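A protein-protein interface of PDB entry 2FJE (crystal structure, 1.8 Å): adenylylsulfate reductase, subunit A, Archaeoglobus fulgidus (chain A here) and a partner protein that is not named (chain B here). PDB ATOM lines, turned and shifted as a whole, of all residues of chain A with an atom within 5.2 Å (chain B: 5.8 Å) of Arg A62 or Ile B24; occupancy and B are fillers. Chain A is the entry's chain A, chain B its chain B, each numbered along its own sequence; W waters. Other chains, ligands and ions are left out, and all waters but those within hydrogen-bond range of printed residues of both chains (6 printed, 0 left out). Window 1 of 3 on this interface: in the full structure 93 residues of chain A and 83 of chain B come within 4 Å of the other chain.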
ATOM      1  N   ALA A  59      -7.451 -13.840  -5.220  1.00  0.00           N
ATOM      2  CA  ALA A  59      -6.663 -14.996  -4.789  1.00  0.00           C
ATOM      3  C   ALA A  59      -5.438 -15.118  -5.693  1.00  0.00           C
ATOM      4  O   ALA A  59      -5.561 -15.189  -6.915  1.00  0.00           O
ATOM      5  CB  ALA A  59      -7.503 -16.266  -4.851  1.00  0.00           C
ATOM      6  N   VAL A  60      -4.259 -15.155  -5.080  1.00  0.00           N
ATOM      7  CA  VAL A  60      -2.999 -15.223  -5.814  1.00  0.00           C
ATOM      8  C   VAL A  60      -2.874 -16.344  -6.847  1.00  0.00           C
ATOM      9  O   VAL A  60      -2.208 -16.174  -7.865  1.00  0.00           O
ATOM     10  CB  VAL A  60      -1.816 -15.305  -4.835  1.00  0.00           C
ATOM     11  CG1 VAL A  60      -0.502 -15.312  -5.601  1.00  0.00           C
ATOM     12  CG2 VAL A  60      -1.866 -14.118  -3.878  1.00  0.00           C
ATOM     13  N   GLU A  61      -3.515 -17.479  -6.591  1.00  0.00           N
ATOM     14  CA  GLU A  61      -3.452 -18.608  -7.511  1.00  0.00           C
ATOM     15  C   GLU A  61      -3.787 -18.223  -8.954  1.00  0.00           C
ATOM     16  O   GLU A  61      -3.163 -18.720  -9.890  1.00  0.00           O
ATOM     17  CB  GLU A  61      -4.402 -19.722  -7.054  1.00  0.00           C
ATOM     18  CG  GLU A  61      -4.184 -21.039  -7.791  1.00  0.00           C
ATOM     19  CD  GLU A  61      -5.099 -22.152  -7.310  1.00  0.00           C
ATOM     20  OE1 GLU A  61      -5.566 -22.089  -6.151  1.00  0.00           O
ATOM     21  OE2 GLU A  61      -5.338 -23.097  -8.088  1.00  0.00           O
ATOM     22  N   ARG A  62      -4.759 -17.331  -9.133  1.00  0.00           N
ATOM     23  CA  ARG A  62      -5.176 -16.920 -10.476  1.00  0.00           C
ATOM     24  C   ARG A  62      -5.365 -15.418 -10.666  1.00  0.00           C
ATOM     25  O   ARG A  62      -5.824 -14.987 -11.722  1.00  0.00           O
ATOM     26  CB  ARG A  62      -6.498 -17.605 -10.836  1.00  0.00           C
ATOM     27  CG  ARG A  62      -6.395 -19.092 -11.094  1.00  0.00           C
ATOM     28  CD  ARG A  62      -5.914 -19.372 -12.501  1.00  0.00           C
ATOM     29  NE  ARG A  62      -5.704 -20.800 -12.711  1.00  0.00           N
ATOM     30  CZ  ARG A  62      -5.363 -21.342 -13.874  1.00  0.00           C
ATOM     31  NH1 ARG A  62      -5.197 -20.573 -14.944  1.00  0.00           N
ATOM     32  NH2 ARG A  62      -5.173 -22.651 -13.960  1.00  0.00           N
ATOM     33  N   SER A  63      -5.001 -14.623  -9.667  1.00  0.00           N
ATOM     34  CA  SER A  63      -5.203 -13.181  -9.747  1.00  0.00           C
ATOM     35  C   SER A  63      -4.385 -12.445 -10.808  1.00  0.00           C
ATOM     36  O   SER A  63      -3.261 -12.831 -11.137  1.00  0.00           O
ATOM     37  CB  SER A  63      -4.946 -12.544  -8.377  1.00  0.00           C
ATOM     38  OG  SER A  63      -3.572 -12.602  -8.031  1.00  0.00           O
ATOM     39  N   GLY A  64      -4.973 -11.385 -11.354  1.00  0.00           N
ATOM     40  CA  GLY A  64      -4.270 -10.589 -12.344  1.00  0.00           C
ATOM     41  C   GLY A  64      -4.400 -10.966 -13.806  1.00  0.00           C
ATOM     42  O   GLY A  64      -5.173 -11.841 -14.191  1.00  0.00           O
ATOM     43  N   VAL A  66      -2.662 -12.701 -15.748  1.00  0.00           N
ATOM     44  CA  VAL A  66      -2.353 -14.070 -16.154  1.00  0.00           C
ATOM     45  C   VAL A  66      -3.340 -15.123 -15.644  1.00  0.00           C
ATOM     46  O   VAL A  66      -3.027 -16.312 -15.594  1.00  0.00           O
ATOM     47  CB  VAL A  66      -0.905 -14.429 -15.723  1.00  0.00           C
ATOM     48  CG1 VAL A  66      -0.482 -15.775 -16.303  1.00  0.00           C
ATOM     49  CG2 VAL A  66       0.047 -13.338 -16.211  1.00  0.00           C
ATOM     50  N   ALA A  67      -4.548 -14.691 -15.296  1.00  0.00           N
ATOM     51  CA  ALA A  67      -5.571 -15.609 -14.800  1.00  0.00           C
ATOM     52  C   ALA A  67      -5.862 -16.791 -15.735  1.00  0.00           C
ATOM     53  O   ALA A  67      -6.067 -17.913 -15.272  1.00  0.00           O
ATOM     54  CB  ALA A  67      -6.863 -14.847 -14.521  1.00  0.00           C
ATOM     55  N   GLN A  68      -5.891 -16.551 -17.043  1.00  0.00           N
ATOM     56  CA  GLN A  68      -6.186 -17.630 -17.994  1.00  0.00           C
ATOM     57  C   GLN A  68      -4.918 -18.345 -18.418  1.00  0.00           C
ATOM     58  O   GLN A  68      -4.968 -19.428 -19.014  1.00  0.00           O
ATOM     59  CB  GLN A  68      -6.851 -17.083 -19.262  1.00  0.00           C
ATOM     60  CG  GLN A  68      -7.793 -15.916 -19.059  1.00  0.00           C
ATOM     61  CD  GLN A  68      -8.620 -15.633 -20.297  1.00  0.00           C
ATOM     62  OE1 GLN A  68      -9.066 -14.503 -20.519  1.00  0.00           O
ATOM     63  NE2 GLN A  68      -8.841 -16.664 -21.109  1.00  0.00           N
ATOM     64  N   GLY A  69      -3.787 -17.722 -18.104  1.00  0.00           N
ATOM     65  CA  GLY A  69      -2.496 -18.247 -18.490  1.00  0.00           C
ATOM     66  C   GLY A  69      -2.025 -17.365 -19.632  1.00  0.00           C
ATOM     67  O   GLY A  69      -2.660 -16.355 -19.938  1.00  0.00           O
ATOM     68  N   GLU A 151      -1.018 -22.492 -19.493  1.00  0.00           N
ATOM     69  CA  GLU A 151      -2.336 -22.431 -18.868  1.00  0.00           C
ATOM     70  C   GLU A 151      -2.203 -22.242 -17.356  1.00  0.00           C
ATOM     71  O   GLU A 151      -2.976 -21.503 -16.746  1.00  0.00           O
ATOM     72  CB  GLU A 151      -3.130 -23.708 -19.166  1.00  0.00           C
ATOM     73  CG  GLU A 151      -4.562 -23.685 -18.639  1.00  0.00           C
ATOM     74  CD  GLU A 151      -4.662 -24.051 -17.170  1.00  0.00           C
ATOM     75  OE1 GLU A 151      -5.611 -23.588 -16.506  1.00  0.00           O
ATOM     76  OE2 GLU A 151      -3.804 -24.815 -16.683  1.00  0.00           O
ATOM     77  N   SER A 152      -1.212 -22.901 -16.758  1.00  0.00           N
ATOM     78  CA  SER A 152      -0.994 -22.806 -15.316  1.00  0.00           C
ATOM     79  C   SER A 152       0.158 -21.882 -14.941  1.00  0.00           C
ATOM     80  O   SER A 152       0.758 -22.026 -13.878  1.00  0.00           O
ATOM     81  CB  SER A 152      -0.738 -24.196 -14.728  1.00  0.00           C
ATOM     82  OG  SER A 152      -1.904 -24.990 -14.793  1.00  0.00           O
ATOM     83  N   LYS A 154       0.193 -18.719 -13.969  1.00  0.00           N
ATOM     84  CA  LYS A 154       0.003 -17.996 -12.711  1.00  0.00           C
ATOM     85  C   LYS A 154       0.086 -18.908 -11.489  1.00  0.00           C
ATOM     86  O   LYS A 154       0.771 -18.586 -10.517  1.00  0.00           O
ATOM     87  CB  LYS A 154      -1.332 -17.243 -12.680  1.00  0.00           C
ATOM     88  CG  LYS A 154      -1.482 -16.403 -11.412  1.00  0.00           C
ATOM     89  CD  LYS A 154      -0.424 -15.294 -11.355  1.00  0.00           C
ATOM     90  CE  LYS A 154      -0.312 -14.667  -9.965  1.00  0.00           C
ATOM     91  NZ  LYS A 154      -1.604 -14.117  -9.460  1.00  0.00           N
ATOM     92  N   PRO A 155      -0.622 -20.047 -11.510  1.00  0.00           N
ATOM     93  CA  PRO A 155      -0.584 -20.971 -10.370  1.00  0.00           C
ATOM     94  C   PRO A 155       0.836 -21.419 -10.021  1.00  0.00           C
ATOM     95  O   PRO A 155       1.171 -21.599  -8.845  1.00  0.00           O
ATOM     96  CB  PRO A 155      -1.458 -22.131 -10.841  1.00  0.00           C
ATOM     97  CG  PRO A 155      -2.483 -21.438 -11.690  1.00  0.00           C
ATOM     98  CD  PRO A 155      -1.637 -20.473 -12.494  1.00  0.00           C
ATOM     99  N   ARG A 173      -8.177 -11.492  -0.592  1.00  0.00           N
ATOM    100  CA  ARG A 173      -9.502 -10.891  -0.487  1.00  0.00           C
ATOM    101  C   ARG A 173      -9.487  -9.660   0.410  1.00  0.00           C
ATOM    102  O   ARG A 173     -10.420  -9.411   1.178  1.00  0.00           O
ATOM    103  CB  ARG A 173     -10.527 -11.915   0.013  1.00  0.00           C
ATOM    104  CG  ARG A 173     -10.730 -13.086  -0.946  1.00  0.00           C
ATOM    105  CD  ARG A 173     -11.229 -12.634  -2.325  1.00  0.00           C
ATOM    106  NE  ARG A 173     -11.169 -13.726  -3.296  1.00  0.00           N
ATOM    107  CZ  ARG A 173     -11.558 -13.637  -4.566  1.00  0.00           C
ATOM    108  NH1 ARG A 173     -12.047 -12.497  -5.043  1.00  0.00           N
ATOM    109  NH2 ARG A 173     -11.450 -14.690  -5.365  1.00  0.00           N
ATOM    110  N   THR B  19     -15.423 -22.797  -0.866  1.00  0.00           N
ATOM    111  CA  THR B  19     -16.178 -22.766  -2.111  1.00  0.00           C
ATOM    112  C   THR B  19     -15.177 -22.435  -3.215  1.00  0.00           C
ATOM    113  O   THR B  19     -14.679 -21.314  -3.293  1.00  0.00           O
ATOM    114  CB  THR B  19     -17.269 -21.680  -2.076  1.00  0.00           C
ATOM    115  OG1 THR B  19     -18.146 -21.919  -0.968  1.00  0.00           O
ATOM    116  CG2 THR B  19     -18.073 -21.691  -3.368  1.00  0.00           C
ATOM    117  N   ALA B  20     -14.886 -23.420  -4.060  1.00  0.00           N
ATOM    118  CA  ALA B  20     -13.919 -23.266  -5.145  1.00  0.00           C
ATOM    119  C   ALA B  20     -14.104 -22.046  -6.048  1.00  0.00           C
ATOM    120  O   ALA B  20     -13.197 -21.224  -6.172  1.00  0.00           O
ATOM    121  CB  ALA B  20     -13.899 -24.533  -5.992  1.00  0.00           C
ATOM    122  N   CYS B  21     -15.264 -21.928  -6.687  1.00  0.00           N
ATOM    123  CA  CYS B  21     -15.518 -20.805  -7.589  1.00  0.00           C
ATOM    124  C   CYS B  21     -15.394 -19.447  -6.899  1.00  0.00           C
ATOM    125  O   CYS B  21     -14.768 -18.525  -7.432  1.00  0.00           O
ATOM    126  CB  CYS B  21     -16.903 -20.940  -8.234  1.00  0.00           C
ATOM    127  SG  CYS B  21     -18.301 -20.954  -7.084  1.00  0.00           S
ATOM    128  N   GLU B  22     -15.988 -19.323  -5.715  1.00  0.00           N
ATOM    129  CA  GLU B  22     -15.930 -18.075  -4.964  1.00  0.00           C
ATOM    130  C   GLU B  22     -14.490 -17.751  -4.584  1.00  0.00           C
ATOM    131  O   GLU B  22     -14.067 -16.596  -4.609  1.00  0.00           O
ATOM    132  CB  GLU B  22     -16.789 -18.181  -3.700  1.00  0.00           C
ATOM    133  CG  GLU B  22     -16.661 -16.990  -2.759  1.00  0.00           C
ATOM    134  CD  GLU B  22     -17.590 -17.090  -1.563  1.00  0.00           C
ATOM    135  OE1 GLU B  22     -17.533 -16.203  -0.685  1.00  0.00           O
ATOM    136  OE2 GLU B  22     -18.379 -18.059  -1.505  1.00  0.00           O
ATOM    137  N   TYR B  23     -13.738 -18.788  -4.238  1.00  0.00           N
ATOM    138  CA  TYR B  23     -12.345 -18.629  -3.850  1.00  0.00           C
ATOM    139  C   TYR B  23     -11.413 -18.184  -4.978  1.00  0.00           C
ATOM    140  O   TYR B  23     -10.546 -17.339  -4.768  1.00  0.00           O
ATOM    141  CB  TYR B  23     -11.821 -19.949  -3.266  1.00  0.00           C
ATOM    142  CG  TYR B  23     -10.320 -20.116  -3.383  1.00  0.00           C
ATOM    143  CD1 TYR B  23      -9.448 -19.362  -2.597  1.00  0.00           C
ATOM    144  CD2 TYR B  23      -9.770 -20.988  -4.324  1.00  0.00           C
ATOM    145  CE1 TYR B  23      -8.064 -19.471  -2.750  1.00  0.00           C
ATOM    146  CE2 TYR B  23      -8.394 -21.102  -4.485  1.00  0.00           C
ATOM    147  CZ  TYR B  23      -7.546 -20.342  -3.697  1.00  0.00           C
ATOM    148  OH  TYR B  23      -6.182 -20.447  -3.866  1.00  0.00           O
ATOM    149  N   ILE B  24     -11.606 -18.731  -6.175  1.00  0.00           N
ATOM    150  CA  ILE B  24     -10.711 -18.440  -7.294  1.00  0.00           C
ATOM    151  C   ILE B  24     -10.960 -17.197  -8.158  1.00  0.00           C
ATOM    152  O   ILE B  24     -10.009 -16.633  -8.704  1.00  0.00           O
ATOM    153  CB  ILE B  24     -10.632 -19.672  -8.239  1.00  0.00           C
ATOM    154  CG1 ILE B  24      -9.325 -19.647  -9.036  1.00  0.00           C
ATOM    155  CG2 ILE B  24     -11.825 -19.685  -9.193  1.00  0.00           C
ATOM    156  CD1 ILE B  24      -8.094 -19.945  -8.196  1.00  0.00           C
ATOM    157  N   CYS B  25     -12.214 -16.770  -8.287  1.00  0.00           N
ATOM    158  CA  CYS B  25     -12.535 -15.622  -9.142  1.00  0.00           C
ATOM    159  C   CYS B  25     -11.724 -14.352  -8.901  1.00  0.00           C
ATOM    160  O   CYS B  25     -11.830 -13.718  -7.849  1.00  0.00           O
ATOM    161  CB  CYS B  25     -14.019 -15.275  -9.054  1.00  0.00           C
ATOM    162  SG  CYS B  25     -14.452 -13.932 -10.189  1.00  0.00           S
ATOM    163  N   PRO B  26     -10.918 -13.949  -9.896  1.00  0.00           N
ATOM    164  CA  PRO B  26     -10.076 -12.753  -9.813  1.00  0.00           C
ATOM    165  C   PRO B  26     -10.845 -11.438  -9.713  1.00  0.00           C
ATOM    166  O   PRO B  26     -10.269 -10.415  -9.344  1.00  0.00           O
ATOM    167  CB  PRO B  26      -9.239 -12.827 -11.092  1.00  0.00           C
ATOM    168  CG  PRO B  26      -9.230 -14.296 -11.425  1.00  0.00           C
ATOM    169  CD  PRO B  26     -10.651 -14.683 -11.145  1.00  0.00           C
ATOM    170  N   ASN B  27     -12.133 -11.450 -10.048  1.00  0.00           N
ATOM    171  CA  ASN B  27     -12.923 -10.226  -9.977  1.00  0.00           C
ATOM    172  C   ASN B  27     -14.045 -10.289  -8.936  1.00  0.00           C
ATOM    173  O   ASN B  27     -14.949  -9.456  -8.941  1.00  0.00           O
ATOM    174  CB  ASN B  27     -13.496  -9.883 -11.361  1.00  0.00           C
ATOM    175  CG  ASN B  27     -13.412  -8.389 -11.678  1.00  0.00           C
ATOM    176  OD1 ASN B  27     -12.695  -7.639 -11.012  1.00  0.00           O
ATOM    177  ND2 ASN B  27     -14.133  -7.959 -12.706  1.00  0.00           N
ATOM    178  N   SER B  52     -11.403 -19.455 -14.839  1.00  0.00           N
ATOM    179  CA  SER B  52     -10.797 -19.935 -13.604  1.00  0.00           C
ATOM    180  C   SER B  52     -11.815 -20.730 -12.797  1.00  0.00           C
ATOM    181  O   SER B  52     -11.535 -21.847 -12.363  1.00  0.00           O
ATOM    182  CB  SER B  52     -10.264 -18.767 -12.771  1.00  0.00           C
ATOM    183  OG  SER B  52      -9.132 -18.184 -13.394  1.00  0.00           O
ATOM    184  N   CYS B  53     -13.001 -20.156 -12.613  1.00  0.00           N
ATOM    185  CA  CYS B  53     -14.057 -20.825 -11.860  1.00  0.00           C
ATOM    186  C   CYS B  53     -14.425 -22.153 -12.517  1.00  0.00           C
ATOM    187  O   CYS B  53     -14.571 -23.171 -11.839  1.00  0.00           O
ATOM    188  CB  CYS B  53     -15.296 -19.926 -11.765  1.00  0.00           C
ATOM    189  SG  CYS B  53     -15.982 -19.402 -13.360  1.00  0.00           S
ATOM    190  N   LYS B  55     -12.654 -24.169 -14.398  1.00  0.00           N
ATOM    191  CA  LYS B  55     -11.602 -25.154 -14.185  1.00  0.00           C
ATOM    192  C   LYS B  55     -11.523 -25.699 -12.764  1.00  0.00           C
ATOM    193  O   LYS B  55     -11.200 -26.870 -12.562  1.00  0.00           O
ATOM    194  CB  LYS B  55     -10.248 -24.544 -14.544  1.00  0.00           C
ATOM    195  CG  LYS B  55     -10.120 -24.069 -15.978  1.00  0.00           C
ATOM    196  CD  LYS B  55      -8.839 -23.288 -16.168  1.00  0.00           C
ATOM    197  CE  LYS B  55      -8.687 -22.785 -17.590  1.00  0.00           C
ATOM    198  NZ  LYS B  55      -7.507 -21.883 -17.705  1.00  0.00           N
ATOM    199  N   MET B  56     -11.820 -24.860 -11.778  1.00  0.00           N
ATOM    200  CA  MET B  56     -11.708 -25.282 -10.387  1.00  0.00           C
ATOM    201  C   MET B  56     -12.936 -25.901  -9.735  1.00  0.00           C
ATOM    202  O   MET B  56     -12.864 -26.364  -8.596  1.00  0.00           O
ATOM    203  CB  MET B  56     -11.203 -24.112  -9.543  1.00  0.00           C
ATOM    204  CG  MET B  56      -9.950 -23.471 -10.120  1.00  0.00           C
ATOM    205  SD  MET B  56      -8.717 -24.685 -10.656  1.00  0.00           S
ATOM    206  CE  MET B  56      -7.300 -24.057  -9.895  1.00  0.00           C
ATOM    207  N   ARG B  81      -9.125 -29.893 -16.715  1.00  0.00           N
ATOM    208  CA  ARG B  81      -7.772 -29.656 -16.246  1.00  0.00           C
ATOM    209  C   ARG B  81      -7.288 -30.735 -15.290  1.00  0.00           C
ATOM    210  O   ARG B  81      -7.941 -31.029 -14.291  1.00  0.00           O
ATOM    211  CB  ARG B  81      -7.725 -28.283 -15.573  1.00  0.00           C
ATOM    212  CG  ARG B  81      -6.363 -27.820 -15.130  1.00  0.00           C
ATOM    213  CD  ARG B  81      -6.404 -26.333 -14.808  1.00  0.00           C
ATOM    214  NE  ARG B  81      -5.143 -25.867 -14.247  1.00  0.00           N
ATOM    215  CZ  ARG B  81      -4.792 -26.025 -12.975  1.00  0.00           C
ATOM    216  NH1 ARG B  81      -5.615 -26.629 -12.129  1.00  0.00           N
ATOM    217  NH2 ARG B  81      -3.615 -25.588 -12.552  1.00  0.00           N
HETATM  218  O   HOH W   1      -8.022 -14.738  -8.026  1.00  0.00           O
HETATM  219  O   HOH W   2      -8.291 -19.867 -15.987  1.00  0.00           O
HETATM  220  O   HOH W   3     -10.435 -16.239  -2.231  1.00  0.00           O
HETATM  221  O   HOH W   4      -6.917 -21.070 -20.161  1.00  0.00           O
HETATM  222  O   HOH W   5      -7.266 -10.321  -9.878  1.00  0.00           O
HETATM  223  O   HOH W   6      -4.426 -18.401  -3.959  1.00  0.00           O
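OE2 of Glu A151 lies within salt-bridge range of NE of Arg B81 (3.0 Å). The side-chain hydroxyl (OH) of Tyr B23 sits at hydrogen-bond distance from the side-chain carboxylate (OE1) of Glu A61, 2.9 Å away. The guanidinium group (NE) of Arg B81 sits close to the guanidinium group (NH2) of Arg A62 (3.2 Å). The side-chain carboxylate of Glu A151 is in salt-bridge range of the side-chain amino group of Lys B55 (2.8 Å). The backbone carbonyl oxygen (O) of Tyr B23 sits at hydrogen-bond distance from the guanidinium group (NH2) of Arg A173 (2.9 Å). NH2 of Arg A173 lies within hydrogen-bond range of O of Glu B22 (3.3 Å). The side-chain hydroxyl of Ser A152 sits at hydrogen-bond distance from the guanidinium group of Arg B81, at 2.9 Å. The guanidinium group (NH2) of Arg A173 lies within hydrogen-bond range of the backbone carbonyl oxygen (O) of Cys B25 (2.7 Å).
The guanidinium group of Arg A62 is in salt-bridge range of the side-chain carboxylate of Glu A151 (2.7 Å). O of Ala A59 lies close to OG of Ser A63, at 3.4 Å. OE2 of Glu A151 sits at hydrogen-bond distance from OG of Ser A152, 2.7 Å away. O of Ala A67 is in hydrogen-bond range of NH1 of Arg A62 (2.8 Å). SG of Cys B25 sits close to N of Asn B27.
O of Tyr B23 touches CB of Ala A59, at 3.2 Å. CD of Glu A61 touches CD1 of Ile B24, 3.8 Å away. CD1 of Ile B24 touches CG of Arg A62, 3.5 Å away. Arg A62 touches Pro B26. OG of Ser B52 touches CD of Arg A62 (3.5 Å). Arg A62 touches Lys B55. Ala A67 touches Pro B26 (CB to CG, 3.9 Å). Ala A67 touches Ser B52. Gln A68 touches Lys B55. Arg A173 touches Ile B24 (NH2 to C, 3.8 Å).
Printed residues of chain B within 4 Å of Ala A59: Tyr B23 (3.2 Å). Arg A62 touches just these residues of chain B: Ile B24, Pro B26, Ser B52, Lys B55 and Arg B81. Of the printed residues of chain B, Ser A152 touches Arg B81 (2.9 Å). Ile B24 touches three residues of chain A. Cys B53 touches none of the printed residues of chain A. The nearest residue of chain B that does not touch Arg A62 is Met B56 (4.6 Å). The nearest residue of chain A that does not touch Ile B24 is Ala A59 (4.6 Å).
Printed residues of chain A that touch a printed residue of chain B: Ala A59, Glu A61, Arg A62, Ala A67, Gln A68, Glu A151, Ser A152 and Arg A173. Hydrophobic or aromatic side chains of chain A within 4 Å of the printed part of chain B: Ala A59 and Ala A67. Hydrophobic or aromatic side chains of chain B within 4 Å of the printed part of chain A: Tyr B23, Ile B24, Pro B26 and Met B56. Along chain B the printed residues that touch a printed residue of chain A span positions 22 to 81. Among the printed residues, 19 pairs touch across the chains.
Water W4 lies within hydrogen-bond range of NZ of Lys B55 (2.7 Å) and O of Gln A68 (2.8 Å). Water W6 lies within hydrogen-bond range of OH of Tyr B23, N of Glu A61 and N of Val A60. Water W1 lies within hydrogen-bond range of O of Ala A59 (2.7 Å), O of Ile B24 (2.8 Å) and N of Ser A63 (3.4 Å). Water W2 lies within hydrogen-bond range of NZ of Lys B55 (2.8 Å), O of Ala A67 (3.0 Å), OG of Ser B52 (3.2 Å) and NH1 of Arg A62 (3.3 Å). Water W3 bridges the backbone carbonyl oxygen (O) of Tyr B23 (2.8 Å) and the guanidinium group (NE) of Arg A173 (2.8 Å). Water W5 bridges the backbone NH of Gly A64 (2.9 Å) and the backbone carbonyl oxygen of Pro B26 (3.1 Å).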
